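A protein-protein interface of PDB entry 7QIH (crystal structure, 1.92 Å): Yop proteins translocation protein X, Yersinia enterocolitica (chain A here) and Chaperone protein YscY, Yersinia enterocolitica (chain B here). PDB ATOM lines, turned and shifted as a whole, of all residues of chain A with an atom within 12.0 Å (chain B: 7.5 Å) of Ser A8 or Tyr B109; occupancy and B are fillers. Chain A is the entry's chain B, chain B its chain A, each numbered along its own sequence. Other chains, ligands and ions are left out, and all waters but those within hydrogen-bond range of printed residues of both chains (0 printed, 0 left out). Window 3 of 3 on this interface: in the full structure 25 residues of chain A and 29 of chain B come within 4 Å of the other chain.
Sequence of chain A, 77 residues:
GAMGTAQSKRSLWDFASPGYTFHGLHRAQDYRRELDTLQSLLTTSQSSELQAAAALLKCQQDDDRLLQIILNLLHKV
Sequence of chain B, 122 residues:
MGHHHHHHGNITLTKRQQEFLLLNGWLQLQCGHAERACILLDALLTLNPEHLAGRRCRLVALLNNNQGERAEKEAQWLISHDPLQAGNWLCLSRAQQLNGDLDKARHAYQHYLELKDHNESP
The guanidinium group (NH1) of Arg B94 sits close to the side-chain amide nitrogen (NE2) of Gln B97 (3.2 Å).
OH of Tyr B112 sits at hydrogen-bond distance from NZ of Lys B116, 3.4 Å away.
The backbone carbonyl oxygen (O) of Gln A7 lies within hydrogen-bond range of the side-chain hydroxyl (OG) of Ser A11 (2.9 Å).
Among the printed residues, merely in contact across the chains: Ser A11 with Leu B90, Ser A8 with Leu B90, Ser A8 with Tyr B109, Leu A12 with Leu B90, Leu A12 with Arg B94 and Ser A11 with Tyr B112.
Printed residues of chain B that touch a printed residue of chain A: Leu B90, Arg B94, Tyr B109 and Tyr B112.
Hydrophobic or aromatic side chains of chain B within 4 Å of the printed part of chain A: Leu B90, Tyr B109 and Tyr B112.
Of the 13 printed residues of chain A, 3 touch a printed residue of chain B.
Hydrophobic or aromatic side chains of chain A that line the printed part of chain B: Leu A12.
Of chain B, only Leu B90 and Tyr B109 come within 4 Å of Ser A8.
Of the printed residues of chain A, Tyr B109 touches Ser A8.
Leu B90 touches just these residues of chain A: Ser A8 (3.7 Å), Ser A11 (3.7 Å) and Leu A12 (3.8 Å).
No residue of chain A comes within 4 Å of Ser B93.
No residue of chain A comes within 4 Å of Ala B108.
Gln B110 touches none of the printed residues of chain A.
Of chain A, only Ser A11 comes within 4 Å of Tyr B112.
Leu B113 touches none of the printed residues of chain A.
Of the printed residues of chain B, Leu A12 touches Leu B90 and Arg B94.
Printed residues of chain B within 4 Å of Ser A11: Leu B90 and Tyr B112.
Printed residues of chain A within 4 Å of Arg B94: Leu A12.
Gln A7 touches none of the printed residues of chain B.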
ATOM      1  N   THR A   5      11.152  22.182   2.093  1.00  0.00           N
ATOM      2  CA  THR A   5      12.083  21.668   1.096  1.00  0.00           C
ATOM      3  C   THR A   5      11.329  21.026  -0.061  1.00  0.00           C
ATOM      4  O   THR A   5      10.385  20.264   0.151  1.00  0.00           O
ATOM      5  CB  THR A   5      13.054  20.637   1.705  1.00  0.00           C
ATOM      6  OG1 THR A   5      13.741  21.224   2.817  1.00  0.00           O
ATOM      7  CG2 THR A   5      14.075  20.182   0.672  1.00  0.00           C
ATOM      8  N   ALA A   6      11.746  21.345  -1.289  1.00  0.00           N
ATOM      9  CA  ALA A   6      11.117  20.745  -2.460  1.00  0.00           C
ATOM     10  C   ALA A   6      11.312  19.234  -2.480  1.00  0.00           C
ATOM     11  O   ALA A   6      10.417  18.492  -2.903  1.00  0.00           O
ATOM     12  CB  ALA A   6      11.674  21.375  -3.738  1.00  0.00           C
ATOM     13  N   GLN A   7      12.475  18.760  -2.026  1.00  0.00           N
ATOM     14  CA  GLN A   7      12.722  17.320  -1.987  1.00  0.00           C
ATOM     15  C   GLN A   7      11.777  16.624  -1.016  1.00  0.00           C
ATOM     16  O   GLN A   7      11.275  15.531  -1.302  1.00  0.00           O
ATOM     17  CB  GLN A   7      14.174  17.040  -1.604  1.00  0.00           C
ATOM     18  CG  GLN A   7      14.502  15.558  -1.529  1.00  0.00           C
ATOM     19  CD  GLN A   7      15.772  15.275  -0.755  1.00  0.00           C
ATOM     20  OE1 GLN A   7      16.397  16.183  -0.207  1.00  0.00           O
ATOM     21  NE2 GLN A   7      16.160  14.006  -0.703  1.00  0.00           N
ATOM     22  N   SER A   8      11.531  17.237   0.145  1.00  0.00           N
ATOM     23  CA  SER A   8      10.580  16.663   1.091  1.00  0.00           C
ATOM     24  C   SER A   8       9.173  16.644   0.506  1.00  0.00           C
ATOM     25  O   SER A   8       8.426  15.677   0.695  1.00  0.00           O
ATOM     26  CB  SER A   8      10.605  17.442   2.407  1.00  0.00           C
ATOM     27  OG  SER A   8      11.871  17.342   3.035  1.00  0.00           O
ATOM     28  N   LYS A   9       8.800  17.704  -0.215  1.00  0.00           N
ATOM     29  CA  LYS A   9       7.484  17.740  -0.844  1.00  0.00           C
ATOM     30  C   LYS A   9       7.352  16.654  -1.904  1.00  0.00           C
ATOM     31  O   LYS A   9       6.311  15.992  -1.998  1.00  0.00           O
ATOM     32  CB  LYS A   9       7.230  19.121  -1.447  1.00  0.00           C
ATOM     33  CG  LYS A   9       7.231  20.249  -0.426  1.00  0.00           C
ATOM     34  CD  LYS A   9       6.994  21.598  -1.085  1.00  0.00           C
ATOM     35  CE  LYS A   9       7.070  22.725  -0.068  1.00  0.00           C
ATOM     36  NZ  LYS A   9       6.886  24.062  -0.698  1.00  0.00           N
ATOM     37  N   ARG A  10       8.398  16.451  -2.710  1.00  0.00           N
ATOM     38  CA  ARG A  10       8.375  15.356  -3.676  1.00  0.00           C
ATOM     39  C   ARG A  10       8.323  14.008  -2.970  1.00  0.00           C
ATOM     40  O   ARG A  10       7.626  13.090  -3.421  1.00  0.00           O
ATOM     41  CB  ARG A  10       9.595  15.428  -4.597  1.00  0.00           C
ATOM     42  CG  ARG A  10       9.631  16.649  -5.502  1.00  0.00           C
ATOM     43  CD  ARG A  10      10.638  16.469  -6.631  1.00  0.00           C
ATOM     44  NE  ARG A  10      11.955  16.083  -6.139  1.00  0.00           N
ATOM     45  CZ  ARG A  10      12.931  16.936  -5.861  1.00  0.00           C
ATOM     46  NH1 ARG A  10      12.779  18.239  -6.024  1.00  0.00           N
ATOM     47  NH2 ARG A  10      14.091  16.468  -5.407  1.00  0.00           N
ATOM     48  N   SER A  11       9.050  13.869  -1.859  1.00  0.00           N
ATOM     49  CA  SER A  11       8.976  12.640  -1.078  1.00  0.00           C
ATOM     50  C   SER A  11       7.580  12.440  -0.499  1.00  0.00           C
ATOM     51  O   SER A  11       7.108  11.304  -0.377  1.00  0.00           O
ATOM     52  CB  SER A  11      10.022  12.659   0.035  1.00  0.00           C
ATOM     53  OG  SER A  11      11.329  12.755  -0.498  1.00  0.00           O
ATOM     54  N   LEU A  12       6.907  13.534  -0.134  1.00  0.00           N
ATOM     55  CA  LEU A  12       5.524  13.440   0.329  1.00  0.00           C
ATOM     56  C   LEU A  12       4.603  12.965  -0.789  1.00  0.00           C
ATOM     57  O   LEU A  12       3.779  12.063  -0.590  1.00  0.00           O
ATOM     58  CB  LEU A  12       5.055  14.791   0.870  1.00  0.00           C
ATOM     59  CG  LEU A  12       5.507  15.176   2.278  1.00  0.00           C
ATOM     60  CD1 LEU A  12       5.025  16.576   2.630  1.00  0.00           C
ATOM     61  CD2 LEU A  12       4.995  14.164   3.287  1.00  0.00           C
ATOM     62  N   TRP A  13       4.720  13.570  -1.974  1.00  0.00           N
ATOM     63  CA  TRP A  13       3.889  13.153  -3.102  1.00  0.00           C
ATOM     64  C   TRP A  13       4.159  11.702  -3.481  1.00  0.00           C
ATOM     65  O   TRP A  13       3.230  10.961  -3.825  1.00  0.00           O
ATOM     66  CB  TRP A  13       4.120  14.075  -4.299  1.00  0.00           C
ATOM     67  CG  TRP A  13       3.371  15.370  -4.207  1.00  0.00           C
ATOM     68  CD1 TRP A  13       3.880  16.594  -3.880  1.00  0.00           C
ATOM     69  CD2 TRP A  13       1.970  15.568  -4.439  1.00  0.00           C
ATOM     70  NE1 TRP A  13       2.883  17.541  -3.898  1.00  0.00           N
ATOM     71  CE2 TRP A  13       1.701  16.937  -4.239  1.00  0.00           C
ATOM     72  CE3 TRP A  13       0.918  14.720  -4.800  1.00  0.00           C
ATOM     73  CZ2 TRP A  13       0.424  17.477  -4.387  1.00  0.00           C
ATOM     74  CZ3 TRP A  13      -0.350  15.258  -4.946  1.00  0.00           C
ATOM     75  CH2 TRP A  13      -0.586  16.623  -4.740  1.00  0.00           C
ATOM     76  N   ASP A  14       5.423  11.276  -3.423  1.00  0.00           N
ATOM     77  CA  ASP A  14       5.739   9.875  -3.680  1.00  0.00           C
ATOM     78  C   ASP A  14       5.118   8.975  -2.622  1.00  0.00           C
ATOM     79  O   ASP A  14       4.691   7.852  -2.921  1.00  0.00           O
ATOM     80  CB  ASP A  14       7.254   9.671  -3.734  1.00  0.00           C
ATOM     81  CG  ASP A  14       7.900  10.387  -4.904  1.00  0.00           C
ATOM     82  OD1 ASP A  14       7.198  10.663  -5.902  1.00  0.00           O
ATOM     83  OD2 ASP A  14       9.114  10.671  -4.828  1.00  0.00           O
ATOM     84  N   PHE A  15       5.055   9.454  -1.378  1.00  0.00           N
ATOM     85  CA  PHE A  15       4.430   8.682  -0.308  1.00  0.00           C
ATOM     86  C   PHE A  15       2.919   8.604  -0.494  1.00  0.00           C
ATOM     87  O   PHE A  15       2.305   7.569  -0.210  1.00  0.00           O
ATOM     88  CB  PHE A  15       4.777   9.309   1.043  1.00  0.00           C
ATOM     89  CG  PHE A  15       4.418   8.459   2.225  1.00  0.00           C
ATOM     90  CD1 PHE A  15       4.995   7.212   2.398  1.00  0.00           C
ATOM     91  CD2 PHE A  15       3.532   8.921   3.182  1.00  0.00           C
ATOM     92  CE1 PHE A  15       4.675   6.432   3.494  1.00  0.00           C
ATOM     93  CE2 PHE A  15       3.212   8.149   4.279  1.00  0.00           C
ATOM     94  CZ  PHE A  15       3.786   6.905   4.436  1.00  0.00           C
ATOM     95  N   ALA A  16       2.303   9.687  -0.968  1.00  0.00           N
ATOM     96  CA  ALA A  16       0.859   9.679  -1.176  1.00  0.00           C
ATOM     97  C   ALA A  16       0.463   8.829  -2.374  1.00  0.00           C
ATOM     98  O   ALA A  16      -0.658   8.313  -2.419  1.00  0.00           O
ATOM     99  CB  ALA A  16       0.345  11.106  -1.359  1.00  0.00           C
ATOM    100  N   SER A  17       1.353   8.678  -3.346  1.00  0.00           N
ATOM    101  CA  SER A  17       1.005   7.984  -4.576  1.00  0.00           C
ATOM    102  C   SER A  17       0.680   6.522  -4.285  1.00  0.00           C
ATOM    103  O   SER A  17       1.467   5.838  -3.615  1.00  0.00           O
ATOM    104  CB  SER A  17       2.150   8.076  -5.582  1.00  0.00           C
ATOM    105  OG  SER A  17       1.815   7.405  -6.784  1.00  0.00           O
ATOM    106  N   ALA B  86       9.109   5.177   7.317  1.00  0.00           N
ATOM    107  CA  ALA B  86       9.684   6.518   7.377  1.00  0.00           C
ATOM    108  C   ALA B  86       8.699   7.586   6.923  1.00  0.00           C
ATOM    109  O   ALA B  86       8.622   8.663   7.527  1.00  0.00           O
ATOM    110  CB  ALA B  86      10.954   6.576   6.528  1.00  0.00           C
ATOM    111  N   TRP B  89       6.567   9.518   9.377  1.00  0.00           N
ATOM    112  CA  TRP B  89       7.205  10.537  10.200  1.00  0.00           C
ATOM    113  C   TRP B  89       7.448  11.824   9.427  1.00  0.00           C
ATOM    114  O   TRP B  89       7.388  12.911  10.011  1.00  0.00           O
ATOM    115  CB  TRP B  89       8.514   9.993  10.775  1.00  0.00           C
ATOM    116  CG  TRP B  89       8.285   8.865  11.728  1.00  0.00           C
ATOM    117  CD1 TRP B  89       8.268   7.533  11.435  1.00  0.00           C
ATOM    118  CD2 TRP B  89       8.012   8.970  13.133  1.00  0.00           C
ATOM    119  NE1 TRP B  89       8.014   6.800  12.571  1.00  0.00           N
ATOM    120  CE2 TRP B  89       7.852   7.660  13.626  1.00  0.00           C
ATOM    121  CE3 TRP B  89       7.895  10.044  14.018  1.00  0.00           C
ATOM    122  CZ2 TRP B  89       7.581   7.397  14.966  1.00  0.00           C
ATOM    123  CZ3 TRP B  89       7.622   9.781  15.350  1.00  0.00           C
ATOM    124  CH2 TRP B  89       7.470   8.467  15.811  1.00  0.00           C
ATOM    125  N   LEU B  90       7.726  11.724   8.125  1.00  0.00           N
ATOM    126  CA  LEU B  90       7.784  12.923   7.297  1.00  0.00           C
ATOM    127  C   LEU B  90       6.433  13.626   7.277  1.00  0.00           C
ATOM    128  O   LEU B  90       6.363  14.859   7.358  1.00  0.00           O
ATOM    129  CB  LEU B  90       8.234  12.564   5.878  1.00  0.00           C
ATOM    130  CG  LEU B  90       8.378  13.725   4.891  1.00  0.00           C
ATOM    131  CD1 LEU B  90       9.414  14.724   5.383  1.00  0.00           C
ATOM    132  CD2 LEU B  90       8.737  13.214   3.502  1.00  0.00           C
ATOM    133  N   LEU B  92       4.190  13.500   9.674  1.00  0.00           N
ATOM    134  CA  LEU B  92       4.017  14.122  10.984  1.00  0.00           C
ATOM    135  C   LEU B  92       4.799  15.424  11.074  1.00  0.00           C
ATOM    136  O   LEU B  92       4.301  16.424  11.605  1.00  0.00           O
ATOM    137  CB  LEU B  92       4.452  13.155  12.084  1.00  0.00           C
ATOM    138  CG  LEU B  92       4.291  13.651  13.523  1.00  0.00           C
ATOM    139  CD1 LEU B  92       2.818  13.780  13.887  1.00  0.00           C
ATOM    140  CD2 LEU B  92       5.009  12.731  14.494  1.00  0.00           C
ATOM    141  N   SER B  93       6.024  15.434  10.541  1.00  0.00           N
ATOM    142  CA  SER B  93       6.846  16.638  10.581  1.00  0.00           C
ATOM    143  C   SER B  93       6.207  17.774   9.792  1.00  0.00           C
ATOM    144  O   SER B  93       6.207  18.926  10.239  1.00  0.00           O
ATOM    145  CB  SER B  93       8.243  16.330  10.040  1.00  0.00           C
ATOM    146  OG  SER B  93       9.071  17.477  10.076  1.00  0.00           O
ATOM    147  N   ARG B  94       5.652  17.468   8.616  1.00  0.00           N
ATOM    148  CA  ARG B  94       5.061  18.515   7.788  1.00  0.00           C
ATOM    149  C   ARG B  94       3.797  19.081   8.423  1.00  0.00           C
ATOM    150  O   ARG B  94       3.574  20.296   8.397  1.00  0.00           O
ATOM    151  CB  ARG B  94       4.770  17.974   6.387  1.00  0.00           C
ATOM    152  CG  ARG B  94       4.090  18.971   5.463  1.00  0.00           C
ATOM    153  CD  ARG B  94       4.873  20.273   5.370  1.00  0.00           C
ATOM    154  NE  ARG B  94       4.182  21.266   4.555  1.00  0.00           N
ATOM    155  CZ  ARG B  94       4.541  22.539   4.456  1.00  0.00           C
ATOM    156  NH1 ARG B  94       5.579  23.018   5.122  1.00  0.00           N
ATOM    157  NH2 ARG B  94       3.838  23.352   3.673  1.00  0.00           N
ATOM    158  N   GLN B  96       3.143  19.195  11.616  1.00  0.00           N
ATOM    159  CA  GLN B  96       3.482  19.931  12.830  1.00  0.00           C
ATOM    160  C   GLN B  96       4.087  21.293  12.509  1.00  0.00           C
ATOM    161  O   GLN B  96       3.839  22.267  13.229  1.00  0.00           O
ATOM    162  CB  GLN B  96       4.426  19.099  13.698  1.00  0.00           C
ATOM    163  CG  GLN B  96       3.729  17.942  14.404  1.00  0.00           C
ATOM    164  CD  GLN B  96       4.683  17.065  15.188  1.00  0.00           C
ATOM    165  OE1 GLN B  96       5.862  16.952  14.852  1.00  0.00           O
ATOM    166  NE2 GLN B  96       4.176  16.434  16.242  1.00  0.00           N
ATOM    167  N   GLN B  97       4.878  21.391  11.437  1.00  0.00           N
ATOM    168  CA  GLN B  97       5.416  22.697  11.069  1.00  0.00           C
ATOM    169  C   GLN B  97       4.338  23.590  10.466  1.00  0.00           C
ATOM    170  O   GLN B  97       4.419  24.819  10.579  1.00  0.00           O
ATOM    171  CB  GLN B  97       6.599  22.549  10.111  1.00  0.00           C
ATOM    172  CG  GLN B  97       6.249  22.071   8.711  1.00  0.00           C
ATOM    173  CD  GLN B  97       7.431  22.155   7.761  1.00  0.00           C
ATOM    174  OE1 GLN B  97       7.999  21.135   7.365  1.00  0.00           O
ATOM    175  NE2 GLN B  97       7.807  23.374   7.391  1.00  0.00           N
ATOM    176  N   ASP B 103       9.593  22.947  16.766  1.00  0.00           N
ATOM    177  CA  ASP B 103      10.521  22.098  17.508  1.00  0.00           C
ATOM    178  C   ASP B 103      10.075  20.641  17.485  1.00  0.00           C
ATOM    179  O   ASP B 103      10.908  19.731  17.403  1.00  0.00           O
ATOM    180  CB  ASP B 103      10.660  22.602  18.944  1.00  0.00           C
ATOM    181  CG  ASP B 103      11.954  22.154  19.597  1.00  0.00           C
ATOM    182  OD1 ASP B 103      13.036  22.523  19.088  1.00  0.00           O
ATOM    183  OD2 ASP B 103      11.893  21.441  20.619  1.00  0.00           O
ATOM    184  N   LYS B 104       8.764  20.400  17.547  1.00  0.00           N
ATOM    185  CA  LYS B 104       8.270  19.034  17.416  1.00  0.00           C
ATOM    186  C   LYS B 104       8.412  18.527  15.987  1.00  0.00           C
ATOM    187  O   LYS B 104       8.629  17.328  15.774  1.00  0.00           O
ATOM    188  CB  LYS B 104       6.811  18.948  17.868  1.00  0.00           C
ATOM    189  CG  LYS B 104       6.586  19.354  19.317  1.00  0.00           C
ATOM    190  CD  LYS B 104       5.404  18.614  19.927  1.00  0.00           C
ATOM    191  CE  LYS B 104       4.136  18.822  19.119  1.00  0.00           C
ATOM    192  NZ  LYS B 104       2.971  18.126  19.735  1.00  0.00           N
ATOM    193  N   ALA B 105       8.301  19.418  14.999  1.00  0.00           N
ATOM    194  CA  ALA B 105       8.465  19.004  13.611  1.00  0.00           C
ATOM    195  C   ALA B 105       9.900  18.587  13.318  1.00  0.00           C
ATOM    196  O   ALA B 105      10.139  17.792  12.401  1.00  0.00           O
ATOM    197  CB  ALA B 105       8.036  20.127  12.669  1.00  0.00           C
ATOM    198  N   ARG B 106      10.864  19.107  14.078  1.00  0.00           N
ATOM    199  CA  ARG B 106      12.252  18.714  13.866  1.00  0.00           C
ATOM    200  C   ARG B 106      12.544  17.350  14.481  1.00  0.00           C
ATOM    201  O   ARG B 106      13.321  16.570  13.919  1.00  0.00           O
ATOM    202  CB  ARG B 106      13.197  19.776  14.430  1.00  0.00           C
ATOM    203  CG  ARG B 106      13.068  21.127  13.745  1.00  0.00           C
ATOM    204  CD  ARG B 106      14.310  21.979  13.940  1.00  0.00           C
ATOM    205  NE  ARG B 106      14.228  23.225  13.185  1.00  0.00           N
ATOM    206  CZ  ARG B 106      14.535  23.345  11.901  1.00  0.00           C
ATOM    207  NH1 ARG B 106      14.944  22.308  11.187  1.00  0.00           N
ATOM    208  NH2 ARG B 106      14.425  24.534  11.316  1.00  0.00           N
ATOM    209  N   HIS B 107      11.934  17.045  15.629  1.00  0.00           N
ATOM    210  CA  HIS B 107      12.089  15.715  16.209  1.00  0.00           C
ATOM    211  C   HIS B 107      11.468  14.652  15.314  1.00  0.00           C
ATOM    212  O   HIS B 107      12.044  13.575  15.124  1.00  0.00           O
ATOM    213  CB  HIS B 107      11.467  15.666  17.605  1.00  0.00           C
ATOM    214  CG  HIS B 107      12.222  16.449  18.631  1.00  0.00           C
ATOM    215  ND1 HIS B 107      12.010  17.793  18.847  1.00  0.00           N
ATOM    216  CD2 HIS B 107      13.190  16.078  19.501  1.00  0.00           C
ATOM    217  CE1 HIS B 107      12.812  18.216  19.808  1.00  0.00           C
ATOM    218  NE2 HIS B 107      13.540  17.193  20.221  1.00  0.00           N
ATOM    219  N   ALA B 108      10.288  14.939  14.754  1.00  0.00           N
ATOM    220  CA  ALA B 108       9.662  13.998  13.832  1.00  0.00           C
ATOM    221  C   ALA B 108      10.508  13.810  12.582  1.00  0.00           C
ATOM    222  O   ALA B 108      10.631  12.692  12.068  1.00  0.00           O
ATOM    223  CB  ALA B 108       8.258  14.475  13.461  1.00  0.00           C
ATOM    224  N   TYR B 109      11.107  14.894  12.079  1.00  0.00           N
ATOM    225  CA  TYR B 109      11.932  14.789  10.880  1.00  0.00           C
ATOM    226  C   TYR B 109      13.198  13.986  11.142  1.00  0.00           C
ATOM    227  O   TYR B 109      13.681  13.285  10.247  1.00  0.00           O
ATOM    228  CB  TYR B 109      12.283  16.182  10.355  1.00  0.00           C
ATOM    229  CG  TYR B 109      12.926  16.169   8.985  1.00  0.00           C
ATOM    230  CD1 TYR B 109      12.152  16.048   7.838  1.00  0.00           C
ATOM    231  CD2 TYR B 109      14.303  16.277   8.840  1.00  0.00           C
ATOM    232  CE1 TYR B 109      12.732  16.033   6.585  1.00  0.00           C
ATOM    233  CE2 TYR B 109      14.892  16.264   7.588  1.00  0.00           C
ATOM    234  CZ  TYR B 109      14.101  16.141   6.466  1.00  0.00           C
ATOM    235  OH  TYR B 109      14.679  16.129   5.218  1.00  0.00           O
ATOM    236  N   GLN B 110      13.749  14.078  12.355  1.00  0.00           N
ATOM    237  CA  GLN B 110      14.905  13.260  12.705  1.00  0.00           C
ATOM    238  C   GLN B 110      14.542  11.780  12.713  1.00  0.00           C
ATOM    239  O   GLN B 110      15.342  10.934  12.293  1.00  0.00           O
ATOM    240  CB  GLN B 110      15.459  13.690  14.064  1.00  0.00           C
ATOM    241  CG  GLN B 110      16.834  13.124  14.384  1.00  0.00           C
ATOM    242  CD  GLN B 110      17.481  13.804  15.574  1.00  0.00           C
ATOM    243  OE1 GLN B 110      16.944  13.791  16.682  1.00  0.00           O
ATOM    244  NE2 GLN B 110      18.641  14.411  15.349  1.00  0.00           N
ATOM    245  N   HIS B 111      13.337  11.451  13.185  1.00  0.00           N
ATOM    246  CA  HIS B 111      12.853  10.076  13.106  1.00  0.00           C
ATOM    247  C   HIS B 111      12.721   9.627  11.660  1.00  0.00           C
ATOM    248  O   HIS B 111      13.022   8.474  11.329  1.00  0.00           O
ATOM    249  CB  HIS B 111      11.509   9.947  13.825  1.00  0.00           C
ATOM    250  CG  HIS B 111      11.624   9.824  15.312  1.00  0.00           C
ATOM    251  ND1 HIS B 111      12.701   9.228  15.931  1.00  0.00           N
ATOM    252  CD2 HIS B 111      10.791  10.219  16.305  1.00  0.00           C
ATOM    253  CE1 HIS B 111      12.529   9.261  17.240  1.00  0.00           C
ATOM    254  NE2 HIS B 111      11.378   9.856  17.494  1.00  0.00           N
ATOM    255  N   TYR B 112      12.254  10.522  10.785  1.00  0.00           N
ATOM    256  CA  TYR B 112      12.191  10.210   9.363  1.00  0.00           C
ATOM    257  C   TYR B 112      13.572   9.885   8.810  1.00  0.00           C
ATOM    258  O   TYR B 112      13.736   8.919   8.054  1.00  0.00           O
ATOM    259  CB  TYR B 112      11.565  11.380   8.603  1.00  0.00           C
ATOM    260  CG  TYR B 112      11.783  11.345   7.106  1.00  0.00           C
ATOM    261  CD1 TYR B 112      11.185  10.369   6.322  1.00  0.00           C
ATOM    262  CD2 TYR B 112      12.572  12.299   6.477  1.00  0.00           C
ATOM    263  CE1 TYR B 112      11.374  10.338   4.957  1.00  0.00           C
ATOM    264  CE2 TYR B 112      12.766  12.276   5.109  1.00  0.00           C
ATOM    265  CZ  TYR B 112      12.166  11.291   4.355  1.00  0.00           C
ATOM    266  OH  TYR B 112      12.354  11.258   2.992  1.00  0.00           O
ATOM    267  N   LEU B 113      14.582  10.674   9.187  1.00  0.00           N
ATOM    268  CA  LEU B 113      15.938  10.419   8.708  1.00  0.00           C
ATOM    269  C   LEU B 113      16.485   9.107   9.257  1.00  0.00           C
ATOM    270  O   LEU B 113      17.235   8.405   8.568  1.00  0.00           O
ATOM    271  CB  LEU B 113      16.857  11.578   9.088  1.00  0.00           C
ATOM    272  CG  LEU B 113      16.528  12.939   8.474  1.00  0.00           C
ATOM    273  CD1 LEU B 113      17.419  14.021   9.060  1.00  0.00           C
ATOM    274  CD2 LEU B 113      16.667  12.890   6.958  1.00  0.00           C
ATOM    275  N   GLU B 114      16.129   8.763  10.498  1.00  0.00           N
ATOM    276  CA  GLU B 114      16.644   7.537  11.102  1.00  0.00           C
ATOM    277  C   GLU B 114      16.073   6.293  10.433  1.00  0.00           C
ATOM    278  O   GLU B 114      16.715   5.236  10.446  1.00  0.00           O
ATOM    279  CB  GLU B 114      16.337   7.522  12.602  1.00  0.00           C
ATOM    280  CG  GLU B 114      17.126   8.555  13.400  1.00  0.00           C
ATOM    281  CD  GLU B 114      16.668   8.671  14.845  1.00  0.00           C
ATOM    282  OE1 GLU B 114      15.680   8.005  15.214  1.00  0.00           O
ATOM    283  OE2 GLU B 114      17.295   9.430  15.612  1.00  0.00           O
ATOM    284  N   LEU B 115      14.887   6.400   9.833  1.00  0.00           N
ATOM    285  CA  LEU B 115      14.187   5.254   9.268  1.00  0.00           C
ATOM    286  C   LEU B 115      14.203   5.196   7.748  1.00  0.00           C
ATOM    287  O   LEU B 115      13.930   4.129   7.189  1.00  0.00           O
ATOM    288  CB  LEU B 115      12.722   5.248   9.735  1.00  0.00           C
ATOM    289  CG  LEU B 115      12.490   5.167  11.245  1.00  0.00           C
ATOM    290  CD1 LEU B 115      11.037   5.483  11.578  1.00  0.00           C
ATOM    291  CD2 LEU B 115      12.879   3.794  11.774  1.00  0.00           C
ATOM    292  N   LYS B 116      14.518   6.295   7.068  1.00  0.00           N
ATOM    293  CA  LYS B 116      14.338   6.346   5.625  1.00  0.00           C
ATOM    294  C   LYS B 116      15.379   5.498   4.902  1.00  0.00           C
ATOM    295  O   LYS B 116      16.454   5.188   5.426  1.00  0.00           O
ATOM    296  CB  LYS B 116      14.413   7.787   5.119  1.00  0.00           C
ATOM    297  CG  LYS B 116      15.791   8.415   5.235  1.00  0.00           C
ATOM    298  CD  LYS B 116      15.844   9.759   4.525  1.00  0.00           C
ATOM    299  CE  LYS B 116      15.669   9.600   3.024  1.00  0.00           C
ATOM    300  NZ  LYS B 116      15.696  10.916   2.326  1.00  0.00           N
